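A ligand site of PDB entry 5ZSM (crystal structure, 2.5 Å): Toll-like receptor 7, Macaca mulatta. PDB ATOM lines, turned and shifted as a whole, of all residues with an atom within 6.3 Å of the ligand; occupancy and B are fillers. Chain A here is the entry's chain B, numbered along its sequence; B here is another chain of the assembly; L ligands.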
ATOM      1  N   TYR A 242       7.097  -7.952  14.695  1.00  0.00           N
ATOM      2  CA  TYR A 242       8.290  -8.162  13.898  1.00  0.00           C
ATOM      3  C   TYR A 242       8.048  -9.247  12.823  1.00  0.00           C
ATOM      4  O   TYR A 242       7.649 -10.353  13.113  1.00  0.00           O
ATOM      5  CB  TYR A 242       9.488  -8.534  14.776  1.00  0.00           C
ATOM      6  CG  TYR A 242      10.820  -8.425  14.072  1.00  0.00           C
ATOM      7  CD1 TYR A 242      11.204  -7.260  13.429  1.00  0.00           C
ATOM      8  CD2 TYR A 242      11.727  -9.472  14.086  1.00  0.00           C
ATOM      9  CE1 TYR A 242      12.438  -7.145  12.809  1.00  0.00           C
ATOM     10  CE2 TYR A 242      12.961  -9.371  13.474  1.00  0.00           C
ATOM     11  CZ  TYR A 242      13.309  -8.208  12.804  1.00  0.00           C
ATOM     12  OH  TYR A 242      14.522  -8.116  12.199  1.00  0.00           O
ATOM     13  N   ASN A 243       8.304  -8.878  11.558  1.00  0.00           N
ATOM     14  CA  ASN A 243       8.251  -9.731  10.372  1.00  0.00           C
ATOM     15  C   ASN A 243       6.850 -10.310  10.194  1.00  0.00           C
ATOM     16  O   ASN A 243       6.689 -11.372   9.648  1.00  0.00           O
ATOM     17  CB  ASN A 243       9.308 -10.835  10.405  1.00  0.00           C
ATOM     18  CG  ASN A 243      10.685 -10.365   9.969  1.00  0.00           C
ATOM     19  OD1 ASN A 243      10.788  -9.557   9.051  1.00  0.00           O
ATOM     20  ND2 ASN A 243      11.734 -10.889  10.575  1.00  0.00           N
ATOM     21  N   PHE A 329      12.645 -14.549  20.756  1.00  0.00           N
ATOM     22  CA  PHE A 329      13.975 -13.901  20.708  1.00  0.00           C
ATOM     23  C   PHE A 329      13.847 -12.377  20.839  1.00  0.00           C
ATOM     24  O   PHE A 329      12.946 -11.801  20.308  1.00  0.00           O
ATOM     25  CB  PHE A 329      14.733 -14.271  19.424  1.00  0.00           C
ATOM     26  CG  PHE A 329      14.250 -13.678  18.119  1.00  0.00           C
ATOM     27  CD1 PHE A 329      13.305 -14.319  17.354  1.00  0.00           C
ATOM     28  CD2 PHE A 329      14.846 -12.541  17.589  1.00  0.00           C
ATOM     29  CE1 PHE A 329      12.901 -13.805  16.125  1.00  0.00           C
ATOM     30  CE2 PHE A 329      14.433 -12.023  16.380  1.00  0.00           C
ATOM     31  CZ  PHE A 329      13.460 -12.659  15.645  1.00  0.00           C
ATOM     32  N   GLU A 330      14.815 -11.752  21.527  1.00  0.00           N
ATOM     33  CA  GLU A 330      14.934 -10.311  21.536  1.00  0.00           C
ATOM     34  C   GLU A 330      15.501  -9.823  20.218  1.00  0.00           C
ATOM     35  O   GLU A 330      16.521 -10.336  19.766  1.00  0.00           O
ATOM     36  CB  GLU A 330      15.934  -9.822  22.567  1.00  0.00           C
ATOM     37  CG  GLU A 330      15.583 -10.118  24.014  1.00  0.00           C
ATOM     38  CD  GLU A 330      16.753  -9.768  24.914  1.00  0.00           C
ATOM     39  OE1 GLU A 330      17.193 -10.677  25.645  1.00  0.00           O
ATOM     40  OE2 GLU A 330      17.246  -8.606  24.840  1.00  0.00           O
ATOM     41  N   LEU A 331      14.890  -8.775  19.642  1.00  0.00           N
ATOM     42  CA  LEU A 331      15.333  -8.326  18.349  1.00  0.00           C
ATOM     43  C   LEU A 331      16.791  -7.839  18.478  1.00  0.00           C
ATOM     44  O   LEU A 331      17.180  -7.279  19.484  1.00  0.00           O
ATOM     45  CB  LEU A 331      14.407  -7.237  17.780  1.00  0.00           C
ATOM     46  CG  LEU A 331      12.894  -7.389  17.977  1.00  0.00           C
ATOM     47  CD1 LEU A 331      12.183  -6.324  17.153  1.00  0.00           C
ATOM     48  CD2 LEU A 331      12.368  -8.774  17.629  1.00  0.00           C
ATOM     49  N   GLN A 332      17.599  -8.177  17.483  1.00  0.00           N
ATOM     50  CA  GLN A 332      19.010  -7.813  17.324  1.00  0.00           C
ATOM     51  C   GLN A 332      19.870  -8.426  18.429  1.00  0.00           C
ATOM     52  O   GLN A 332      20.927  -7.933  18.659  1.00  0.00           O
ATOM     53  CB  GLN A 332      19.193  -6.286  17.214  1.00  0.00           C
ATOM     54  CG  GLN A 332      18.628  -5.683  15.928  1.00  0.00           C
ATOM     55  CD  GLN A 332      17.122  -5.482  15.976  1.00  0.00           C
ATOM     56  OE1 GLN A 332      16.599  -4.829  16.878  1.00  0.00           O
ATOM     57  NE2 GLN A 332      16.402  -6.061  15.038  1.00  0.00           N
ATOM     58  N   VAL A 333      19.418  -9.520  19.055  1.00  0.00           N
ATOM     59  CA  VAL A 333      20.266 -10.316  19.931  1.00  0.00           C
ATOM     60  C   VAL A 333      20.369 -11.755  19.422  1.00  0.00           C
ATOM     61  O   VAL A 333      19.373 -12.488  19.285  1.00  0.00           O
ATOM     62  CB  VAL A 333      19.749 -10.321  21.378  1.00  0.00           C
ATOM     63  CG1 VAL A 333      20.637 -11.167  22.269  1.00  0.00           C
ATOM     64  CG2 VAL A 333      19.581  -8.915  21.944  1.00  0.00           C
ATOM     65  N   TYR A 334      21.633 -12.196  19.290  1.00  0.00           N
ATOM     66  CA  TYR A 334      22.020 -13.523  18.898  1.00  0.00           C
ATOM     67  C   TYR A 334      22.751 -14.213  20.064  1.00  0.00           C
ATOM     68  O   TYR A 334      23.974 -14.201  20.123  1.00  0.00           O
ATOM     69  CB  TYR A 334      22.870 -13.397  17.621  1.00  0.00           C
ATOM     70  CG  TYR A 334      23.087 -14.629  16.783  1.00  0.00           C
ATOM     71  CD1 TYR A 334      22.481 -15.865  17.047  1.00  0.00           C
ATOM     72  CD2 TYR A 334      23.872 -14.534  15.654  1.00  0.00           C
ATOM     73  CE1 TYR A 334      22.725 -16.975  16.251  1.00  0.00           C
ATOM     74  CE2 TYR A 334      24.064 -15.622  14.813  1.00  0.00           C
ATOM     75  CZ  TYR A 334      23.506 -16.844  15.117  1.00  0.00           C
ATOM     76  OH  TYR A 334      23.746 -17.880  14.263  1.00  0.00           O
ATOM     77  N   VAL A 359      16.960 -18.324  18.779  1.00  0.00           N
ATOM     78  CA  VAL A 359      18.024 -17.694  17.976  1.00  0.00           C
ATOM     79  C   VAL A 359      19.314 -17.634  18.805  1.00  0.00           C
ATOM     80  O   VAL A 359      19.525 -16.710  19.616  1.00  0.00           O
ATOM     81  CB  VAL A 359      17.618 -16.299  17.450  1.00  0.00           C
ATOM     82  CG1 VAL A 359      18.743 -15.666  16.656  1.00  0.00           C
ATOM     83  CG2 VAL A 359      16.325 -16.329  16.654  1.00  0.00           C
ATOM     84  N   ASN A 385      16.463 -21.479  14.461  1.00  0.00           N
ATOM     85  CA  ASN A 385      17.249 -20.943  15.551  1.00  0.00           C
ATOM     86  C   ASN A 385      18.629 -20.449  15.086  1.00  0.00           C
ATOM     87  O   ASN A 385      19.336 -19.828  15.847  1.00  0.00           O
ATOM     88  CB  ASN A 385      17.393 -21.960  16.683  1.00  0.00           C
ATOM     89  CG  ASN A 385      16.201 -21.900  17.604  1.00  0.00           C
ATOM     90  OD1 ASN A 385      15.892 -20.828  18.110  1.00  0.00           O
ATOM     91  ND2 ASN A 385      15.532 -23.026  17.814  1.00  0.00           N
ATOM     92  N   PHE A 386      18.969 -20.631  13.813  1.00  0.00           N
ATOM     93  CA  PHE A 386      20.273 -20.196  13.274  1.00  0.00           C
ATOM     94  C   PHE A 386      21.435 -20.740  14.125  1.00  0.00           C
ATOM     95  O   PHE A 386      22.442 -20.069  14.317  1.00  0.00           O
ATOM     96  CB  PHE A 386      20.336 -18.683  13.159  1.00  0.00           C
ATOM     97  CG  PHE A 386      19.206 -18.077  12.375  1.00  0.00           C
ATOM     98  CD1 PHE A 386      19.343 -17.841  11.021  1.00  0.00           C
ATOM     99  CD2 PHE A 386      18.038 -17.700  13.022  1.00  0.00           C
ATOM    100  CE1 PHE A 386      18.308 -17.221  10.325  1.00  0.00           C
ATOM    101  CE2 PHE A 386      16.998 -17.098  12.318  1.00  0.00           C
ATOM    102  CZ  PHE A 386      17.135 -16.892  10.980  1.00  0.00           C
ATOM    103  N   LYS A 388      24.674 -22.508  14.711  1.00  0.00           N
ATOM    104  CA  LYS A 388      25.899 -22.704  13.916  1.00  0.00           C
ATOM    105  C   LYS A 388      26.576 -24.025  14.268  1.00  0.00           C
ATOM    106  O   LYS A 388      27.148 -24.608  13.410  1.00  0.00           O
ATOM    107  CB  LYS A 388      26.874 -21.545  14.124  1.00  0.00           C
ATOM    108  CG  LYS A 388      26.371 -20.217  13.571  1.00  0.00           C
ATOM    109  CD  LYS A 388      27.445 -19.183  13.393  1.00  0.00           C
ATOM    110  CE  LYS A 388      27.080 -18.176  12.324  1.00  0.00           C
ATOM    111  NZ  LYS A 388      27.509 -16.809  12.710  1.00  0.00           N
ATOM    112  N   LYS A 410      21.797 -23.290  10.857  1.00  0.00           N
ATOM    113  CA  LYS A 410      23.071 -22.927  10.197  1.00  0.00           C
ATOM    114  C   LYS A 410      24.174 -23.914  10.580  1.00  0.00           C
ATOM    115  O   LYS A 410      25.364 -23.612  10.545  1.00  0.00           O
ATOM    116  CB  LYS A 410      23.429 -21.499  10.586  1.00  0.00           C
ATOM    117  CG  LYS A 410      22.543 -20.401  10.000  1.00  0.00           C
ATOM    118  CD  LYS A 410      23.026 -19.835   8.680  1.00  0.00           C
ATOM    119  CE  LYS A 410      22.054 -18.852   8.072  1.00  0.00           C
ATOM    120  NZ  LYS A 410      22.593 -18.228   6.837  1.00  0.00           N
ATOM    121  N   SER B 508      25.966 -19.227   1.516  1.00  0.00           N
ATOM    122  CA  SER B 508      24.854 -19.287   2.410  1.00  0.00           C
ATOM    123  C   SER B 508      24.972 -18.225   3.501  1.00  0.00           C
ATOM    124  O   SER B 508      24.392 -18.371   4.563  1.00  0.00           O
ATOM    125  CB  SER B 508      24.809 -20.644   3.020  1.00  0.00           C
ATOM    126  OG  SER B 508      24.570 -21.587   2.002  1.00  0.00           O
ATOM    127  N   THR B 510      25.471 -14.329   5.356  1.00  0.00           N
ATOM    128  CA  THR B 510      24.810 -13.043   5.570  1.00  0.00           C
ATOM    129  C   THR B 510      25.757 -11.935   5.088  1.00  0.00           C
ATOM    130  O   THR B 510      26.310 -11.187   5.899  1.00  0.00           O
ATOM    131  CB  THR B 510      24.421 -12.852   7.040  1.00  0.00           C
ATOM    132  OG1 THR B 510      25.480 -13.294   7.896  1.00  0.00           O
ATOM    133  CG2 THR B 510      23.170 -13.601   7.425  1.00  0.00           C
ATOM    134  N   ASP B 533      21.581 -14.974   1.951  1.00  0.00           N
ATOM    135  CA  ASP B 533      20.827 -14.613   3.133  1.00  0.00           C
ATOM    136  C   ASP B 533      20.893 -13.083   3.244  1.00  0.00           C
ATOM    137  O   ASP B 533      21.864 -12.555   3.778  1.00  0.00           O
ATOM    138  CB  ASP B 533      21.412 -15.310   4.368  1.00  0.00           C
ATOM    139  CG  ASP B 533      20.521 -15.263   5.588  1.00  0.00           C
ATOM    140  OD1 ASP B 533      19.601 -14.421   5.606  1.00  0.00           O
ATOM    141  OD2 ASP B 533      20.761 -16.066   6.533  1.00  0.00           O
ATOM    142  N   LEU B 534      19.865 -12.407   2.737  1.00  0.00           N
ATOM    143  CA  LEU B 534      19.786 -10.959   2.740  1.00  0.00           C
ATOM    144  C   LEU B 534      19.339 -10.435   4.110  1.00  0.00           C
ATOM    145  O   LEU B 534      18.379  -9.655   4.184  1.00  0.00           O
ATOM    146  CB  LEU B 534      18.777 -10.518   1.691  1.00  0.00           C
ATOM    147  CG  LEU B 534      19.331  -9.771   0.477  1.00  0.00           C
ATOM    148  CD1 LEU B 534      18.199  -9.070  -0.243  1.00  0.00           C
ATOM    149  CD2 LEU B 534      20.385  -8.764   0.867  1.00  0.00           C
ATOM    150  N   LEU B 535      20.055 -10.787   5.172  1.00  0.00           N
ATOM    151  CA  LEU B 535      19.805 -10.216   6.510  1.00  0.00           C
ATOM    152  C   LEU B 535      20.182  -8.746   6.516  1.00  0.00           C
ATOM    153  O   LEU B 535      19.460  -7.931   7.060  1.00  0.00           O
ATOM    154  CB  LEU B 535      20.651 -10.961   7.542  1.00  0.00           C
ATOM    155  CG  LEU B 535      20.713 -10.314   8.918  1.00  0.00           C
ATOM    156  CD1 LEU B 535      19.308 -10.081   9.512  1.00  0.00           C
ATOM    157  CD2 LEU B 535      21.538 -11.171   9.862  1.00  0.00           C
ATOM    158  N   GLY B 562       9.770 -16.298   9.132  1.00  0.00           N
ATOM    159  CA  GLY B 562      10.383 -15.711  10.300  1.00  0.00           C
ATOM    160  C   GLY B 562      11.810 -15.274  10.072  1.00  0.00           C
ATOM    161  O   GLY B 562      12.457 -14.819  11.022  1.00  0.00           O
ATOM    162  N   ILE B 563      12.307 -15.386   8.834  1.00  0.00           N
ATOM    163  CA  ILE B 563      13.666 -14.950   8.503  1.00  0.00           C
ATOM    164  C   ILE B 563      13.621 -13.514   7.964  1.00  0.00           C
ATOM    165  O   ILE B 563      12.815 -13.178   7.126  1.00  0.00           O
ATOM    166  CB  ILE B 563      14.316 -15.921   7.513  1.00  0.00           C
ATOM    167  CG1 ILE B 563      14.220 -17.350   8.037  1.00  0.00           C
ATOM    168  CG2 ILE B 563      15.763 -15.562   7.225  1.00  0.00           C
ATOM    169  CD1 ILE B 563      15.068 -18.343   7.254  1.00  0.00           C
ATOM    170  N   THR B 564      14.550 -12.682   8.453  1.00  0.00           N
ATOM    171  CA  THR B 564      14.603 -11.258   8.125  1.00  0.00           C
ATOM    172  C   THR B 564      15.314 -11.079   6.786  1.00  0.00           C
ATOM    173  O   THR B 564      16.397 -11.617   6.592  1.00  0.00           O
ATOM    174  CB  THR B 564      15.260 -10.513   9.296  1.00  0.00           C
ATOM    175  OG1 THR B 564      14.348 -10.572  10.392  1.00  0.00           O
ATOM    176  CG2 THR B 564      15.577  -9.073   8.990  1.00  0.00           C
ATOM    177  N   HIS B 565      14.660 -10.386   5.858  1.00  0.00           N
ATOM    178  CA  HIS B 565      15.211 -10.076   4.539  1.00  0.00           C
ATOM    179  C   HIS B 565      15.082  -8.575   4.264  1.00  0.00           C
ATOM    180  O   HIS B 565      14.008  -7.974   4.393  1.00  0.00           O
ATOM    181  CB  HIS B 565      14.503 -10.826   3.406  1.00  0.00           C
ATOM    182  CG  HIS B 565      14.077 -12.239   3.663  1.00  0.00           C
ATOM    183  ND1 HIS B 565      14.979 -13.265   3.898  1.00  0.00           N
ATOM    184  CD2 HIS B 565      12.833 -12.789   3.675  1.00  0.00           C
ATOM    185  CE1 HIS B 565      14.307 -14.378   4.083  1.00  0.00           C
ATOM    186  NE2 HIS B 565      12.972 -14.109   3.945  1.00  0.00           N
HETATM  187  O1  LIG L   1      22.441 -16.022   9.982  1.00  0.00           O
HETATM  188  C1  LIG L   1      21.397 -15.383  10.157  1.00  0.00           C
HETATM  189  C2  LIG L   1      21.039 -14.990  11.543  1.00  0.00           C
HETATM  190  N1  LIG L   1      21.577 -15.120  12.779  1.00  0.00           N
HETATM  191  C3  LIG L   1      20.717 -14.479  13.593  1.00  0.00           C
HETATM  192  N2  LIG L   1      20.558 -15.045   9.141  1.00  0.00           N
HETATM  193  C4  LIG L   1      19.398 -14.347   9.349  1.00  0.00           C
HETATM  194  N3  LIG L   1      18.570 -13.965   8.328  1.00  0.00           N
HETATM  195  N4  LIG L   1      19.068 -13.954  10.576  1.00  0.00           N
HETATM  196  C5  LIG L   1      19.808 -14.218  11.655  1.00  0.00           C
HETATM  197  N5  LIG L   1      19.669 -13.949  12.925  1.00  0.00           N
HETATM  198  C6  LIG L   1      18.534 -13.198  13.461  1.00  0.00           C
HETATM  199  C7  LIG L   1      18.419 -11.820  12.816  1.00  0.00           C
HETATM  200  O2  LIG L   1      18.787 -10.711  13.658  1.00  0.00           O
HETATM  201  O3  LIG L   1      17.331 -13.903  13.203  1.00  0.00           O
HETATM  202  C8  LIG L   1      16.261 -12.948  13.015  1.00  0.00           C
HETATM  203  C9  LIG L   1      15.185 -13.460  12.048  1.00  0.00           C
HETATM  204  O4  LIG L   1      15.850 -13.875  10.860  1.00  0.00           O
HETATM  205  C10 LIG L   1      16.936 -11.700  12.473  1.00  0.00           C
HETATM  206  O5  LIG L   1      16.408 -10.528  13.073  1.00  0.00           O
HETATM  207  P1  LIG L   1      17.534  -9.745  13.874  1.00  0.00           P
HETATM  208  O6  LIG L   1      17.210  -9.959  15.326  1.00  0.00           O
HETATM  209  O7  LIG L   1      17.673  -8.313  13.344  1.00  0.00           O
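Phe 329 touches the ligand (CE2 to O6, 3.6 Å). C of Leu 331 touches O6 of the ligand (3.8 Å). Tyr 334 touches the ligand (CE2 to N1, 3.3 Å). Val 359 touches the ligand (CG1 to C3, 3.8 Å). CE1 of Phe 386 touches C4 of the ligand, 3.2 Å away. Lys 410 touches the ligand (CE to O1, 3.4 Å). Thr 510 of chain B touches the ligand (CG2 to N2, 3.4 Å). CB of Leu 535 of chain B touches N3 of the ligand, at 3.7 Å. Gly 562 of chain B touches the ligand. Ile 563 of chain B touches the ligand (CA to O4, 3.4 Å). Hydrophobic or aromatic side chains within 4 Å of the ligand: Tyr 242, Phe 329, Tyr 334, Val 359, Phe 386, Leu 535 of chain B and Ile 563 of chain B.
The side-chain carboxylate (OD2) of Asp 533 of chain B is in salt-bridge range of the side-chain amino group (NZ) of Lys 410 (2.9 Å). OH of Tyr 242 sits at hydrogen-bond distance from OG1 of Thr 564 of chain B (3.1 Å). ND2 of Asn 243 sits at hydrogen-bond distance from OG1 of Thr 564 of chain B. O of Phe 386 lies within hydrogen-bond range of OH of Tyr 334, 2.5 Å away. A ring nitrogen (NE2) of His 565 of chain B sits at hydrogen-bond distance from the backbone carbonyl oxygen (O) of Ile 563 of chain B (3.3 Å). NZ of Lys 410 is in hydrogen-bond range of O of Ser 508 of chain B, at 2.9 Å. The side-chain amide oxygen (OD1) of Asn 385 lies within hydrogen-bond range of the backbone NH (N) of Val 359, at 2.8 Å.
The side-chain carboxylate (OD2) of Asp 533 of chain B lies within hydrogen-bond range of a nitrogen (N2) of the ligand (2.8 Å). The backbone NH (N) of Gln 332 lies within hydrogen-bond range of an oxygen (O6) of the ligand, at 2.8 Å. The side-chain amide nitrogen (NE2) of Gln 332 sits at hydrogen-bond distance from an oxygen (O7) of the ligand (3.1 Å). N of Thr 564 of chain B sits at hydrogen-bond distance from O4 of the ligand (3.0 Å). OG1 of Thr 564 of chain B is in hydrogen-bond range of O5 of the ligand (3.4 Å). The side-chain hydroxyl of Tyr 242 sits at hydrogen-bond distance from an oxygen (O5) of the ligand.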
